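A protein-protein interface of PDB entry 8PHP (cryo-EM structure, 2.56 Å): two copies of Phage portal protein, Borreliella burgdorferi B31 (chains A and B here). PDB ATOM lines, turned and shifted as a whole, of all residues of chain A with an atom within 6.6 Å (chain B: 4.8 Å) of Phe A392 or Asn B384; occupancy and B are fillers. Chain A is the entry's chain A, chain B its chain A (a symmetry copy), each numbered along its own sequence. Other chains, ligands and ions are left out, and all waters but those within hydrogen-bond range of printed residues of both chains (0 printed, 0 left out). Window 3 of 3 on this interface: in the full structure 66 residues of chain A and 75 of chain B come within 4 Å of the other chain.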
ATOM      1  N   LEU A 386      -3.454  18.385 -20.392  1.00  0.00           N
ATOM      2  CA  LEU A 386      -4.684  17.703 -19.998  1.00  0.00           C
ATOM      3  C   LEU A 386      -5.539  18.578 -19.090  1.00  0.00           C
ATOM      4  O   LEU A 386      -6.760  18.651 -19.259  1.00  0.00           O
ATOM      5  CB  LEU A 386      -4.352  16.382 -19.307  1.00  0.00           C
ATOM      6  CG  LEU A 386      -5.534  15.612 -18.713  1.00  0.00           C
ATOM      7  CD1 LEU A 386      -6.567  15.298 -19.783  1.00  0.00           C
ATOM      8  CD2 LEU A 386      -5.061  14.340 -18.029  1.00  0.00           C
ATOM      9  N   SER A 389      -7.197  21.619 -21.094  1.00  0.00           N
ATOM     10  CA  SER A 389      -8.139  21.273 -22.154  1.00  0.00           C
ATOM     11  C   SER A 389      -9.071  20.135 -21.749  1.00  0.00           C
ATOM     12  O   SER A 389      -9.377  19.250 -22.550  1.00  0.00           O
ATOM     13  CB  SER A 389      -7.394  20.914 -23.436  1.00  0.00           C
ATOM     14  OG  SER A 389      -6.594  19.759 -23.254  1.00  0.00           O
ATOM     15  N   SER A 390      -9.534  20.142 -20.502  1.00  0.00           N
ATOM     16  CA  SER A 390     -10.485  19.145 -20.033  1.00  0.00           C
ATOM     17  C   SER A 390     -11.499  19.806 -19.113  1.00  0.00           C
ATOM     18  O   SER A 390     -11.278  20.903 -18.593  1.00  0.00           O
ATOM     19  CB  SER A 390      -9.792  17.988 -19.302  1.00  0.00           C
ATOM     20  OG  SER A 390      -9.371  18.383 -18.008  1.00  0.00           O
ATOM     21  N   SER A 391     -12.619  19.119 -18.918  1.00  0.00           N
ATOM     22  CA  SER A 391     -13.699  19.575 -18.053  1.00  0.00           C
ATOM     23  C   SER A 391     -14.003  18.537 -16.979  1.00  0.00           C
ATOM     24  O   SER A 391     -15.159  18.306 -16.618  1.00  0.00           O
ATOM     25  CB  SER A 391     -14.951  19.892 -18.866  1.00  0.00           C
ATOM     26  OG  SER A 391     -15.363  18.768 -19.624  1.00  0.00           O
ATOM     27  N   PHE A 392     -12.960  17.896 -16.460  1.00  0.00           N
ATOM     28  CA  PHE A 392     -13.134  16.901 -15.415  1.00  0.00           C
ATOM     29  C   PHE A 392     -13.548  17.559 -14.105  1.00  0.00           C
ATOM     30  O   PHE A 392     -13.187  18.702 -13.813  1.00  0.00           O
ATOM     31  CB  PHE A 392     -11.844  16.106 -15.211  1.00  0.00           C
ATOM     32  CG  PHE A 392     -11.628  15.024 -16.228  1.00  0.00           C
ATOM     33  CD1 PHE A 392     -12.506  13.958 -16.322  1.00  0.00           C
ATOM     34  CD2 PHE A 392     -10.545  15.070 -17.089  1.00  0.00           C
ATOM     35  CE1 PHE A 392     -12.309  12.960 -17.257  1.00  0.00           C
ATOM     36  CE2 PHE A 392     -10.342  14.076 -18.025  1.00  0.00           C
ATOM     37  CZ  PHE A 392     -11.225  13.019 -18.109  1.00  0.00           C
ATOM     38  N   ASN A 393     -14.321  16.823 -13.312  1.00  0.00           N
ATOM     39  CA  ASN A 393     -14.737  17.310 -12.008  1.00  0.00           C
ATOM     40  C   ASN A 393     -13.541  17.389 -11.063  1.00  0.00           C
ATOM     41  O   ASN A 393     -12.503  16.757 -11.274  1.00  0.00           O
ATOM     42  CB  ASN A 393     -15.817  16.406 -11.415  1.00  0.00           C
ATOM     43  CG  ASN A 393     -17.141  16.527 -12.140  1.00  0.00           C
ATOM     44  OD1 ASN A 393     -17.440  17.560 -12.740  1.00  0.00           O
ATOM     45  ND2 ASN A 393     -17.943  15.470 -12.088  1.00  0.00           N
ATOM     46  N   ASN A 394     -13.698  18.191 -10.007  1.00  0.00           N
ATOM     47  CA  ASN A 394     -12.618  18.362  -9.043  1.00  0.00           C
ATOM     48  C   ASN A 394     -12.267  17.043  -8.366  1.00  0.00           C
ATOM     49  O   ASN A 394     -11.087  16.731  -8.170  1.00  0.00           O
ATOM     50  CB  ASN A 394     -13.002  19.415  -8.003  1.00  0.00           C
ATOM     51  CG  ASN A 394     -11.816  19.888  -7.185  1.00  0.00           C
ATOM     52  OD1 ASN A 394     -10.678  19.488  -7.431  1.00  0.00           O
ATOM     53  ND2 ASN A 394     -12.077  20.743  -6.204  1.00  0.00           N
ATOM     54  N   GLU A 395     -13.280  16.255  -7.996  1.00  0.00           N
ATOM     55  CA  GLU A 395     -13.019  14.951  -7.396  1.00  0.00           C
ATOM     56  C   GLU A 395     -12.305  14.025  -8.372  1.00  0.00           C
ATOM     57  O   GLU A 395     -11.375  13.305  -7.990  1.00  0.00           O
ATOM     58  CB  GLU A 395     -14.326  14.321  -6.915  1.00  0.00           C
ATOM     59  CG  GLU A 395     -15.110  15.185  -5.943  1.00  0.00           C
ATOM     60  CD  GLU A 395     -16.278  14.449  -5.320  1.00  0.00           C
ATOM     61  OE1 GLU A 395     -16.553  13.305  -5.739  1.00  0.00           O
ATOM     62  OE2 GLU A 395     -16.924  15.015  -4.413  1.00  0.00           O
ATOM     63  N   GLU A 396     -12.732  14.023  -9.638  1.00  0.00           N
ATOM     64  CA  GLU A 396     -12.055  13.207 -10.642  1.00  0.00           C
ATOM     65  C   GLU A 396     -10.625  13.682 -10.865  1.00  0.00           C
ATOM     66  O   GLU A 396      -9.706  12.865 -10.996  1.00  0.00           O
ATOM     67  CB  GLU A 396     -12.841  13.230 -11.953  1.00  0.00           C
ATOM     68  CG  GLU A 396     -14.343  13.096 -11.776  1.00  0.00           C
ATOM     69  CD  GLU A 396     -15.088  13.111 -13.095  1.00  0.00           C
ATOM     70  OE1 GLU A 396     -14.774  13.970 -13.946  1.00  0.00           O
ATOM     71  OE2 GLU A 396     -15.987  12.265 -13.283  1.00  0.00           O
ATOM     72  N   LEU A 397     -10.418  15.000 -10.917  1.00  0.00           N
ATOM     73  CA  LEU A 397      -9.063  15.528 -11.040  1.00  0.00           C
ATOM     74  C   LEU A 397      -8.229  15.194  -9.811  1.00  0.00           C
ATOM     75  O   LEU A 397      -7.050  14.841  -9.928  1.00  0.00           O
ATOM     76  CB  LEU A 397      -9.101  17.040 -11.264  1.00  0.00           C
ATOM     77  CG  LEU A 397      -9.590  17.520 -12.631  1.00  0.00           C
ATOM     78  CD1 LEU A 397      -9.727  19.033 -12.650  1.00  0.00           C
ATOM     79  CD2 LEU A 397      -8.648  17.050 -13.727  1.00  0.00           C
ATOM     80  N   LEU A 400      -7.131  11.462  -9.729  1.00  0.00           N
ATOM     81  CA  LEU A 400      -6.024  11.168 -10.632  1.00  0.00           C
ATOM     82  C   LEU A 400      -4.676  11.455  -9.980  1.00  0.00           C
ATOM     83  O   LEU A 400      -3.673  10.819 -10.326  1.00  0.00           O
ATOM     84  CB  LEU A 400      -6.185  11.975 -11.923  1.00  0.00           C
ATOM     85  CG  LEU A 400      -4.995  12.098 -12.875  1.00  0.00           C
ATOM     86  CD1 LEU A 400      -4.735  10.780 -13.581  1.00  0.00           C
ATOM     87  CD2 LEU A 400      -5.229  13.212 -13.882  1.00  0.00           C
ATOM     88  N   TYR B 380      -6.624   9.363 -19.908  1.00  0.00           N
ATOM     89  CA  TYR B 380      -7.562  10.384 -19.455  1.00  0.00           C
ATOM     90  C   TYR B 380      -7.865  11.386 -20.562  1.00  0.00           C
ATOM     91  O   TYR B 380      -9.007  11.842 -20.698  1.00  0.00           O
ATOM     92  CB  TYR B 380      -7.009  11.095 -18.222  1.00  0.00           C
ATOM     93  CG  TYR B 380      -7.492  10.514 -16.914  1.00  0.00           C
ATOM     94  CD1 TYR B 380      -7.255   9.184 -16.596  1.00  0.00           C
ATOM     95  CD2 TYR B 380      -8.188  11.292 -16.001  1.00  0.00           C
ATOM     96  CE1 TYR B 380      -7.695   8.646 -15.402  1.00  0.00           C
ATOM     97  CE2 TYR B 380      -8.632  10.763 -14.803  1.00  0.00           C
ATOM     98  CZ  TYR B 380      -8.382   9.441 -14.511  1.00  0.00           C
ATOM     99  OH  TYR B 380      -8.822   8.908 -13.321  1.00  0.00           O
ATOM    100  N   SER B 381      -6.853  11.750 -21.352  1.00  0.00           N
ATOM    101  CA  SER B 381      -7.075  12.671 -22.462  1.00  0.00           C
ATOM    102  C   SER B 381      -8.022  12.074 -23.494  1.00  0.00           C
ATOM    103  O   SER B 381      -8.907  12.768 -24.010  1.00  0.00           O
ATOM    104  CB  SER B 381      -5.740  13.042 -23.107  1.00  0.00           C
ATOM    105  OG  SER B 381      -5.934  13.892 -24.224  1.00  0.00           O
ATOM    106  N   LYS B 382      -7.847  10.790 -23.813  1.00  0.00           N
ATOM    107  CA  LYS B 382      -8.746  10.133 -24.757  1.00  0.00           C
ATOM    108  C   LYS B 382     -10.163  10.048 -24.204  1.00  0.00           C
ATOM    109  O   LYS B 382     -11.135  10.246 -24.940  1.00  0.00           O
ATOM    110  CB  LYS B 382      -8.219   8.740 -25.100  1.00  0.00           C
ATOM    111  CG  LYS B 382      -6.955   8.744 -25.940  1.00  0.00           C
ATOM    112  CD  LYS B 382      -7.177   9.448 -27.268  1.00  0.00           C
ATOM    113  CE  LYS B 382      -5.927   9.400 -28.131  1.00  0.00           C
ATOM    114  NZ  LYS B 382      -6.220   9.740 -29.551  1.00  0.00           N
ATOM    115  N   TYR B 383     -10.297   9.747 -22.910  1.00  0.00           N
ATOM    116  CA  TYR B 383     -11.621   9.671 -22.300  1.00  0.00           C
ATOM    117  C   TYR B 383     -12.322  11.024 -22.326  1.00  0.00           C
ATOM    118  O   TYR B 383     -13.524  11.103 -22.602  1.00  0.00           O
ATOM    119  CB  TYR B 383     -11.509   9.157 -20.866  1.00  0.00           C
ATOM    120  CG  TYR B 383     -12.843   8.928 -20.196  1.00  0.00           C
ATOM    121  CD1 TYR B 383     -13.760   8.029 -20.719  1.00  0.00           C
ATOM    122  CD2 TYR B 383     -13.187   9.616 -19.040  1.00  0.00           C
ATOM    123  CE1 TYR B 383     -14.981   7.817 -20.111  1.00  0.00           C
ATOM    124  CE2 TYR B 383     -14.405   9.410 -18.425  1.00  0.00           C
ATOM    125  CZ  TYR B 383     -15.298   8.511 -18.963  1.00  0.00           C
ATOM    126  OH  TYR B 383     -16.513   8.304 -18.352  1.00  0.00           O
ATOM    127  N   ASN B 384     -11.586  12.100 -22.035  1.00  0.00           N
ATOM    128  CA  ASN B 384     -12.181  13.431 -22.065  1.00  0.00           C
ATOM    129  C   ASN B 384     -12.622  13.807 -23.473  1.00  0.00           C
ATOM    130  O   ASN B 384     -13.686  14.408 -23.659  1.00  0.00           O
ATOM    131  CB  ASN B 384     -11.189  14.459 -21.520  1.00  0.00           C
ATOM    132  CG  ASN B 384     -11.681  15.883 -21.678  1.00  0.00           C
ATOM    133  OD1 ASN B 384     -12.506  16.358 -20.899  1.00  0.00           O
ATOM    134  ND2 ASN B 384     -11.175  16.575 -22.692  1.00  0.00           N
ATOM    135  N   GLN B 385     -11.811  13.467 -24.478  1.00  0.00           N
ATOM    136  CA  GLN B 385     -12.170  13.778 -25.857  1.00  0.00           C
ATOM    137  C   GLN B 385     -13.423  13.022 -26.285  1.00  0.00           C
ATOM    138  O   GLN B 385     -14.276  13.571 -26.992  1.00  0.00           O
ATOM    139  CB  GLN B 385     -11.001  13.452 -26.785  1.00  0.00           C
ATOM    140  CG  GLN B 385     -11.214  13.877 -28.226  1.00  0.00           C
ATOM    141  CD  GLN B 385      -9.973  13.691 -29.073  1.00  0.00           C
ATOM    142  OE1 GLN B 385      -8.910  13.332 -28.566  1.00  0.00           O
ATOM    143  NE2 GLN B 385     -10.100  13.935 -30.373  1.00  0.00           N
ATOM    144  N   LEU B 386     -13.545  11.757 -25.874  1.00  0.00           N
ATOM    145  CA  LEU B 386     -14.727  10.976 -26.227  1.00  0.00           C
ATOM    146  C   LEU B 386     -15.989  11.570 -25.616  1.00  0.00           C
ATOM    147  O   LEU B 386     -17.024  11.664 -26.284  1.00  0.00           O
ATOM    148  CB  LEU B 386     -14.549   9.525 -25.780  1.00  0.00           C
ATOM    149  CG  LEU B 386     -15.761   8.609 -25.958  1.00  0.00           C
ATOM    150  CD1 LEU B 386     -16.198   8.566 -27.414  1.00  0.00           C
ATOM    151  CD2 LEU B 386     -15.461   7.210 -25.443  1.00  0.00           C
ATOM    152  N   ILE B 387     -15.924  11.975 -24.346  1.00  0.00           N
ATOM    153  CA  ILE B 387     -17.104  12.510 -23.675  1.00  0.00           C
ATOM    154  C   ILE B 387     -17.547  13.816 -24.325  1.00  0.00           C
ATOM    155  O   ILE B 387     -18.744  14.041 -24.547  1.00  0.00           O
ATOM    156  CB  ILE B 387     -16.823  12.692 -22.172  1.00  0.00           C
ATOM    157  CG1 ILE B 387     -16.597  11.335 -21.504  1.00  0.00           C
ATOM    158  CG2 ILE B 387     -17.967  13.431 -21.498  1.00  0.00           C
ATOM    159  CD1 ILE B 387     -17.802  10.427 -21.545  1.00  0.00           C
ATOM    160  N   GLN B 388     -16.595  14.693 -24.642  1.00  0.00           N
ATOM    161  CA  GLN B 388     -16.940  16.008 -25.173  1.00  0.00           C
ATOM    162  C   GLN B 388     -17.531  15.914 -26.574  1.00  0.00           C
ATOM    163  O   GLN B 388     -18.448  16.670 -26.917  1.00  0.00           O
ATOM    164  CB  GLN B 388     -15.705  16.909 -25.172  1.00  0.00           C
ATOM    165  CG  GLN B 388     -15.315  17.424 -23.798  1.00  0.00           C
ATOM    166  CD  GLN B 388     -14.190  18.437 -23.856  1.00  0.00           C
ATOM    167  OE1 GLN B 388     -13.922  19.026 -24.903  1.00  0.00           O
ATOM    168  NE2 GLN B 388     -13.523  18.645 -22.727  1.00  0.00           N
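Leu A386 touches Tyr B380 (CD2 to CB, 3.8 Å).
Ser B381 touches Leu A386.
Ser A390 touches Asn B384 (CB to OD1, 3.5 Å).
Gln B388 touches Ser A391.
CZ of Phe A392 touches O of Tyr B380, at 3.6 Å.
CE1 of Phe A392 touches CD2 of Tyr B383, 3.9 Å away.
CE2 of Phe A392 touches CB of Asn B384, 3.6 Å away.
Leu A400 touches Tyr B380.
Position printed for both chains: 386.
Of the 10 pairs that touch across the chains among the printed residues, none has its exchanged pair printed and touching as well.
OD1 of Asn B384 is in hydrogen-bond range of NE2 of Gln B388 (3.1 Å).
The side-chain hydroxyl (OG) of Ser A390 sits at hydrogen-bond distance from the backbone carbonyl oxygen (O) of Leu A386 (2.9 Å).
Of the printed residues of chain B, Leu A386 touches Tyr B380 (3.8 Å) and Ser B381 (3.8 Å).
Of the printed residues of chain B, Ser A390 touches Asn B384 (3.5 Å).
Printed residues of chain B within 4 Å of Ser A391: Asn B384 (3.4 Å) and Gln B388 (3.6 Å).
Phe A392 touches three residues of chain B.
Asn B384 touches four residues of chain A.
Leu B386 touches none of the printed residues of chain A.
Printed residues of chain A within 4 Å of Gln B388: Ser A391 (3.6 Å).
The nearest printed residue of chain B that does not touch Phe A392 is Ser B381 (5.4 Å).
The nearest printed residue of chain A that does not touch Tyr B380 is Glu A396 (4.5 Å).
Of the 9 printed residues of chain B, 5 touch a printed residue of chain A.
Hydrophobic or aromatic side chains of chain B within 4 Å of the printed part of chain A: Tyr B380 and Tyr B383.
Along chain B the printed residues that touch a printed residue of chain A span positions 380 to 388.
Among the printed residues, no Asp or Glu carboxylate lies within 4 Å of a Lys or Arg side-chain nitrogen of the other chain.
OD1 of Asn B384 lies within hydrogen-bond range of N of Ser A391 (3.4 Å).
O of Ser A389 is in hydrogen-bond range of ND2 of Asn B384 (3.2 Å).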
